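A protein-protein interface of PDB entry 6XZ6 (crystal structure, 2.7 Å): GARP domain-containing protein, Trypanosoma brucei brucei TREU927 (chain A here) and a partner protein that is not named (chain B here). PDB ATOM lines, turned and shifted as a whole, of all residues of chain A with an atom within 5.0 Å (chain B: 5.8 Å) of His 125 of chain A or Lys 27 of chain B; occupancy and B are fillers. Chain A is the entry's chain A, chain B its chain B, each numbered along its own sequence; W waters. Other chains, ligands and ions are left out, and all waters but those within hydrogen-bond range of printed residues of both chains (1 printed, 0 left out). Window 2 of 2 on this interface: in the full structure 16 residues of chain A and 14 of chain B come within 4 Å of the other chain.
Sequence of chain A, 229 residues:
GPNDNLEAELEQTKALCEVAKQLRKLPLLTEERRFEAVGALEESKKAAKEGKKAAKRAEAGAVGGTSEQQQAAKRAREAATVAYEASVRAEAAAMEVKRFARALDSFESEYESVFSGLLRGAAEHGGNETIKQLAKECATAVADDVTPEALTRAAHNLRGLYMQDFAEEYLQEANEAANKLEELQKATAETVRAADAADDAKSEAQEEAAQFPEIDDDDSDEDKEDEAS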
ATOM      1  N   GLU A   9       1.462  26.232  25.675  1.00  0.00           N
ATOM      2  CA  GLU A   9       2.150  25.003  25.359  1.00  0.00           C
ATOM      3  C   GLU A   9       3.533  24.914  26.009  1.00  0.00           C
ATOM      4  O   GLU A   9       3.971  23.826  26.367  1.00  0.00           O
ATOM      5  CB  GLU A   9       2.196  24.810  23.839  1.00  0.00           C
ATOM      6  CG  GLU A   9       2.742  23.438  23.446  1.00  0.00           C
ATOM      7  CD  GLU A   9       2.964  23.164  21.978  1.00  0.00           C
ATOM      8  OE1 GLU A   9       3.618  22.137  21.688  1.00  0.00           O
ATOM      9  OE2 GLU A   9       2.503  23.965  21.127  1.00  0.00           O
ATOM     10  N   GLY A 121       6.428  13.305  22.196  1.00  0.00           N
ATOM     11  CA  GLY A 121       5.513  13.951  21.257  1.00  0.00           C
ATOM     12  C   GLY A 121       5.839  15.420  21.084  1.00  0.00           C
ATOM     13  O   GLY A 121       5.953  15.882  19.951  1.00  0.00           O
ATOM     14  N   ALA A 122       6.045  16.158  22.208  1.00  0.00           N
ATOM     15  CA  ALA A 122       6.459  17.586  22.232  1.00  0.00           C
ATOM     16  C   ALA A 122       7.872  17.771  21.593  1.00  0.00           C
ATOM     17  O   ALA A 122       8.115  18.789  20.928  1.00  0.00           O
ATOM     18  CB  ALA A 122       6.440  18.129  23.656  1.00  0.00           C
ATOM     19  N   ALA A 123       8.785  16.775  21.748  1.00  0.00           N
ATOM     20  CA  ALA A 123      10.120  16.803  21.131  1.00  0.00           C
ATOM     21  C   ALA A 123      10.048  16.777  19.604  1.00  0.00           C
ATOM     22  O   ALA A 123      10.805  17.491  18.936  1.00  0.00           O
ATOM     23  CB  ALA A 123      10.950  15.631  21.618  1.00  0.00           C
ATOM     24  N   GLU A 124       9.119  15.960  19.062  1.00  0.00           N
ATOM     25  CA  GLU A 124       8.883  15.728  17.633  1.00  0.00           C
ATOM     26  C   GLU A 124       7.914  16.727  16.973  1.00  0.00           C
ATOM     27  O   GLU A 124       8.132  17.101  15.819  1.00  0.00           O
ATOM     28  CB  GLU A 124       8.320  14.316  17.427  1.00  0.00           C
ATOM     29  CG  GLU A 124       9.222  13.184  17.902  1.00  0.00           C
ATOM     30  CD  GLU A 124       8.556  11.837  18.153  1.00  0.00           C
ATOM     31  OE1 GLU A 124       7.363  11.659  17.805  1.00  0.00           O
ATOM     32  OE2 GLU A 124       9.244  10.949  18.709  1.00  0.00           O
ATOM     33  N   HIS A 125       6.824  17.108  17.676  1.00  0.00           N
ATOM     34  CA  HIS A 125       5.753  17.943  17.146  1.00  0.00           C
ATOM     35  C   HIS A 125       5.403  19.186  17.997  1.00  0.00           C
ATOM     36  O   HIS A 125       4.293  19.715  17.880  1.00  0.00           O
ATOM     37  CB  HIS A 125       4.494  17.081  16.893  1.00  0.00           C
ATOM     38  CG  HIS A 125       4.759  15.830  16.116  1.00  0.00           C
ATOM     39  ND1 HIS A 125       5.143  15.872  14.782  1.00  0.00           N
ATOM     40  CD2 HIS A 125       4.723  14.540  16.520  1.00  0.00           C
ATOM     41  CE1 HIS A 125       5.327  14.609  14.417  1.00  0.00           C
ATOM     42  NE2 HIS A 125       5.079  13.768  15.424  1.00  0.00           N
ATOM     43  N   GLY A 126       6.345  19.670  18.801  1.00  0.00           N
ATOM     44  CA  GLY A 126       6.145  20.871  19.612  1.00  0.00           C
ATOM     45  C   GLY A 126       5.946  22.064  18.714  1.00  0.00           C
ATOM     46  O   GLY A 126       6.496  22.093  17.607  1.00  0.00           O
ATOM     47  N   GLY A 127       5.133  23.017  19.170  1.00  0.00           N
ATOM     48  CA  GLY A 127       4.735  24.209  18.415  1.00  0.00           C
ATOM     49  C   GLY A 127       5.831  25.155  17.975  1.00  0.00           C
ATOM     50  O   GLY A 127       5.687  25.812  16.941  1.00  0.00           O
ATOM     51  N   LYS A 132      10.190  22.204  21.528  1.00  0.00           N
ATOM     52  CA  LYS A 132      10.840  20.971  21.036  1.00  0.00           C
ATOM     53  C   LYS A 132      12.183  20.796  21.731  1.00  0.00           C
ATOM     54  O   LYS A 132      12.553  19.655  22.039  1.00  0.00           O
ATOM     55  CB  LYS A 132      11.103  21.023  19.526  1.00  0.00           C
ATOM     56  CG  LYS A 132       9.934  20.714  18.644  1.00  0.00           C
ATOM     57  CD  LYS A 132      10.405  20.737  17.189  1.00  0.00           C
ATOM     58  CE  LYS A 132       9.244  20.669  16.219  1.00  0.00           C
ATOM     59  NZ  LYS A 132       9.584  21.305  14.917  1.00  0.00           N
ATOM     60  N   ARG B  16      -1.670  16.212  23.975  1.00  0.00           N
ATOM     61  CA  ARG B  16      -0.888  17.427  24.084  1.00  0.00           C
ATOM     62  C   ARG B  16      -0.723  18.035  22.670  1.00  0.00           C
ATOM     63  O   ARG B  16      -0.676  17.272  21.699  1.00  0.00           O
ATOM     64  CB  ARG B  16       0.453  17.175  24.805  1.00  0.00           C
ATOM     65  CG  ARG B  16       1.457  16.241  24.109  1.00  0.00           C
ATOM     66  CD  ARG B  16       2.689  17.033  23.648  1.00  0.00           C
ATOM     67  NE  ARG B  16       2.545  17.465  22.252  1.00  0.00           N
ATOM     68  CZ  ARG B  16       2.892  18.655  21.785  1.00  0.00           C
ATOM     69  NH1 ARG B  16       2.683  18.957  20.505  1.00  0.00           N
ATOM     70  NH2 ARG B  16       3.457  19.552  22.590  1.00  0.00           N
ATOM     71  N   PRO B  17      -0.656  19.382  22.513  1.00  0.00           N
ATOM     72  CA  PRO B  17      -0.842  20.406  23.552  1.00  0.00           C
ATOM     73  C   PRO B  17      -2.355  20.561  23.838  1.00  0.00           C
ATOM     74  O   PRO B  17      -3.205  20.058  23.091  1.00  0.00           O
ATOM     75  CB  PRO B  17      -0.214  21.649  22.921  1.00  0.00           C
ATOM     76  CG  PRO B  17      -0.478  21.494  21.465  1.00  0.00           C
ATOM     77  CD  PRO B  17      -0.532  19.999  21.180  1.00  0.00           C
ATOM     78  N   TYR B  22      -7.855  24.431  17.542  1.00  0.00           N
ATOM     79  CA  TYR B  22      -6.747  24.032  16.675  1.00  0.00           C
ATOM     80  C   TYR B  22      -7.078  24.414  15.243  1.00  0.00           C
ATOM     81  O   TYR B  22      -8.243  24.476  14.863  1.00  0.00           O
ATOM     82  CB  TYR B  22      -6.499  22.522  16.787  1.00  0.00           C
ATOM     83  CG  TYR B  22      -6.236  22.067  18.203  1.00  0.00           C
ATOM     84  CD1 TYR B  22      -7.285  21.866  19.097  1.00  0.00           C
ATOM     85  CD2 TYR B  22      -4.938  21.829  18.654  1.00  0.00           C
ATOM     86  CE1 TYR B  22      -7.050  21.476  20.415  1.00  0.00           C
ATOM     87  CE2 TYR B  22      -4.694  21.418  19.965  1.00  0.00           C
ATOM     88  CZ  TYR B  22      -5.759  21.232  20.835  1.00  0.00           C
ATOM     89  OH  TYR B  22      -5.568  20.803  22.115  1.00  0.00           O
ATOM     90  N   GLN B  25      -4.010  21.338   9.919  1.00  0.00           N
ATOM     91  CA  GLN B  25      -2.660  20.750   9.922  1.00  0.00           C
ATOM     92  C   GLN B  25      -1.960  20.800  11.310  1.00  0.00           C
ATOM     93  O   GLN B  25      -0.823  20.340  11.422  1.00  0.00           O
ATOM     94  CB  GLN B  25      -1.760  21.307   8.799  1.00  0.00           C
ATOM     95  CG  GLN B  25      -2.278  21.043   7.373  1.00  0.00           C
ATOM     96  CD  GLN B  25      -2.601  19.589   7.081  1.00  0.00           C
ATOM     97  OE1 GLN B  25      -3.773  19.212   6.956  1.00  0.00           O
ATOM     98  NE2 GLN B  25      -1.573  18.742   6.963  1.00  0.00           N
ATOM     99  N   ASP B  26      -2.670  21.278  12.367  1.00  0.00           N
ATOM    100  CA  ASP B  26      -2.159  21.292  13.742  1.00  0.00           C
ATOM    101  C   ASP B  26      -2.207  19.857  14.232  1.00  0.00           C
ATOM    102  O   ASP B  26      -3.242  19.193  14.088  1.00  0.00           O
ATOM    103  CB  ASP B  26      -3.007  22.190  14.678  1.00  0.00           C
ATOM    104  CG  ASP B  26      -2.637  23.679  14.762  1.00  0.00           C
ATOM    105  OD1 ASP B  26      -1.909  24.173  13.865  1.00  0.00           O
ATOM    106  OD2 ASP B  26      -3.087  24.353  15.726  1.00  0.00           O
ATOM    107  N   LYS B  27      -1.080  19.368  14.770  1.00  0.00           N
ATOM    108  CA  LYS B  27      -0.955  18.006  15.276  1.00  0.00           C
ATOM    109  C   LYS B  27      -0.987  17.931  16.790  1.00  0.00           C
ATOM    110  O   LYS B  27      -0.319  18.715  17.495  1.00  0.00           O
ATOM    111  CB  LYS B  27       0.343  17.328  14.782  1.00  0.00           C
ATOM    112  CG  LYS B  27       0.345  16.928  13.320  1.00  0.00           C
ATOM    113  CD  LYS B  27       1.285  15.789  13.051  1.00  0.00           C
ATOM    114  CE  LYS B  27       1.893  15.916  11.687  1.00  0.00           C
ATOM    115  NZ  LYS B  27       3.196  16.653  11.737  1.00  0.00           N
ATOM    116  N   ILE B  28      -1.736  16.941  17.287  1.00  0.00           N
ATOM    117  CA  ILE B  28      -1.761  16.567  18.695  1.00  0.00           C
ATOM    118  C   ILE B  28      -1.075  15.178  18.796  1.00  0.00           C
ATOM    119  O   ILE B  28      -1.070  14.424  17.824  1.00  0.00           O
ATOM    120  CB  ILE B  28      -3.172  16.602  19.363  1.00  0.00           C
ATOM    121  CG1 ILE B  28      -4.159  15.551  18.777  1.00  0.00           C
ATOM    122  CG2 ILE B  28      -3.770  17.989  19.338  1.00  0.00           C
ATOM    123  CD1 ILE B  28      -4.294  14.237  19.559  1.00  0.00           C
ATOM    124  N   THR B  29      -0.476  14.871  19.946  1.00  0.00           N
ATOM    125  CA  THR B  29       0.103  13.561  20.241  1.00  0.00           C
ATOM    126  C   THR B  29      -0.618  13.068  21.517  1.00  0.00           C
ATOM    127  O   THR B  29      -0.879  13.848  22.412  1.00  0.00           O
ATOM    128  CB  THR B  29       1.641  13.574  20.383  1.00  0.00           C
ATOM    129  OG1 THR B  29       2.006  14.480  21.414  1.00  0.00           O
ATOM    130  CG2 THR B  29       2.367  13.901  19.088  1.00  0.00           C
ATOM    131  N   ASP B  44      -0.218   9.970  16.969  1.00  0.00           N
ATOM    132  CA  ASP B  44      -0.436  11.208  16.220  1.00  0.00           C
ATOM    133  C   ASP B  44      -1.856  11.382  15.717  1.00  0.00           C
ATOM    134  O   ASP B  44      -2.536  10.405  15.402  1.00  0.00           O
ATOM    135  CB  ASP B  44       0.487  11.228  14.995  1.00  0.00           C
ATOM    136  CG  ASP B  44       1.628  12.205  15.088  1.00  0.00           C
ATOM    137  OD1 ASP B  44       1.488  13.216  15.825  1.00  0.00           O
ATOM    138  OD2 ASP B  44       2.665  11.971  14.417  1.00  0.00           O
ATOM    139  N   ALA B  45      -2.283  12.647  15.603  1.00  0.00           N
ATOM    140  CA  ALA B  45      -3.574  13.071  15.050  1.00  0.00           C
ATOM    141  C   ALA B  45      -3.453  14.503  14.546  1.00  0.00           C
ATOM    142  O   ALA B  45      -2.909  15.358  15.243  1.00  0.00           O
ATOM    143  CB  ALA B  45      -4.683  12.948  16.075  1.00  0.00           C
ATOM    144  N   THR B  46      -3.895  14.733  13.299  1.00  0.00           N
ATOM    145  CA  THR B  46      -3.836  16.025  12.612  1.00  0.00           C
ATOM    146  C   THR B  46      -5.245  16.601  12.450  1.00  0.00           C
ATOM    147  O   THR B  46      -6.195  15.844  12.221  1.00  0.00           O
ATOM    148  CB  THR B  46      -3.134  15.859  11.248  1.00  0.00           C
ATOM    149  OG1 THR B  46      -1.947  15.095  11.418  1.00  0.00           O
ATOM    150  CG2 THR B  46      -2.777  17.181  10.599  1.00  0.00           C
ATOM    151  N   CYS B  47      -5.371  17.942  12.575  1.00  0.00           N
ATOM    152  CA  CYS B  47      -6.636  18.636  12.381  1.00  0.00           C
ATOM    153  C   CYS B  47      -6.867  18.805  10.881  1.00  0.00           C
ATOM    154  O   CYS B  47      -6.064  19.437  10.191  1.00  0.00           O
ATOM    155  CB  CYS B  47      -6.650  19.975  13.118  1.00  0.00           C
ATOM    156  SG  CYS B  47      -8.104  21.010  12.780  1.00  0.00           S
ATOM    157  N   TRP B  52     -10.168  15.108  13.523  1.00  0.00           N
ATOM    158  CA  TRP B  52      -8.865  14.563  13.888  1.00  0.00           C
ATOM    159  C   TRP B  52      -8.624  13.309  13.112  1.00  0.00           C
ATOM    160  O   TRP B  52      -9.464  12.403  13.130  1.00  0.00           O
ATOM    161  CB  TRP B  52      -8.751  14.344  15.413  1.00  0.00           C
ATOM    162  CG  TRP B  52      -8.776  15.652  16.155  1.00  0.00           C
ATOM    163  CD1 TRP B  52      -9.864  16.252  16.708  1.00  0.00           C
ATOM    164  CD2 TRP B  52      -7.710  16.609  16.228  1.00  0.00           C
ATOM    165  NE1 TRP B  52      -9.532  17.499  17.178  1.00  0.00           N
ATOM    166  CE2 TRP B  52      -8.211  17.744  16.900  1.00  0.00           C
ATOM    167  CE3 TRP B  52      -6.368  16.603  15.820  1.00  0.00           C
ATOM    168  CZ2 TRP B  52      -7.412  18.866  17.181  1.00  0.00           C
ATOM    169  CZ3 TRP B  52      -5.588  17.724  16.072  1.00  0.00           C
ATOM    170  CH2 TRP B  52      -6.112  18.838  16.746  1.00  0.00           C
HETATM  171  O   HOH W   1       4.982  18.192  13.302  1.00  0.00           O
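A ring nitrogen (NE2) of His 125 of chain A lies within hydrogen-bond range of the side-chain carboxylate of Asp 44 of chain B (3.2 Å).
The guanidinium group (NH2) of Arg 16 of chain B lies within salt-bridge range of the side-chain carboxylate (OE1) of Glu 9 of chain A (2.7 Å).
The guanidinium group (NH1) of Arg 16 of chain B lies within hydrogen-bond range of the backbone carbonyl oxygen (O) of His 125 of chain A, at 3.2 Å.
The side-chain carboxylate of Glu 9 of chain A sits at hydrogen-bond distance from the backbone NH of Gly 127 of chain A, at 3.1 Å.
N of Arg 16 of chain B is in hydrogen-bond range of O of Thr 29 of chain B (2.9 Å).
The backbone carbonyl oxygen (O) of Pro 17 of chain B sits at hydrogen-bond distance from the side-chain hydroxyl (OH) of Tyr 22 of chain B (2.7 Å).
Pro 17 of chain B touches Glu 9 of chain A.
Gly 121 of chain A touches Thr 29 of chain B.
CB of Ala 122 of chain A touches NH2 of Arg 16 of chain B (3.5 Å).
ND1 of His 125 of chain A touches NZ of Lys 27 of chain B, at 3.7 Å.
Thr 29 of chain B touches His 125 of chain A.
Printed residues of chain B within 4 Å of Glu 9 of chain A: Arg 16 and Pro 17.
Of the printed residues of chain B, Gly 121 of chain A touches Thr 29.
Of the printed residues of chain B, Ala 122 of chain A touches Arg 16.
His 125 of chain A touches four residues of chain B.
Gly 126 of chain A touches none of the printed residues of chain B.
Lys 27 of chain B touches one residue of chain A.
Of the printed residues of chain A, Thr 29 of chain B touches Gly 121 and His 125.
Of the printed residues of chain A, Asp 44 of chain B touches His 125.
The nearest printed residue of chain B that does not touch His 125 of chain A is Pro 17 of chain B (5.9 Å).
The nearest printed residue of chain A that does not touch Lys 27 of chain B is Glu 124 of chain A (6.4 Å).
Of the 9 printed residues of chain A, 4 touch a printed residue of chain B.
Of the 13 printed residues of chain B, 5 touch a printed residue of chain A.
Among the printed residues, Asp or Glu carboxylates within 4 Å of a Lys or Arg side-chain nitrogen of the other chain: Glu 9 of chain A with Arg 16 of chain B (2.7 Å).
Water W1 lies within hydrogen-bond range of ND1 of His 125 of chain A (2.8 Å) and NZ of Lys 27 of chain B (2.8 Å).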
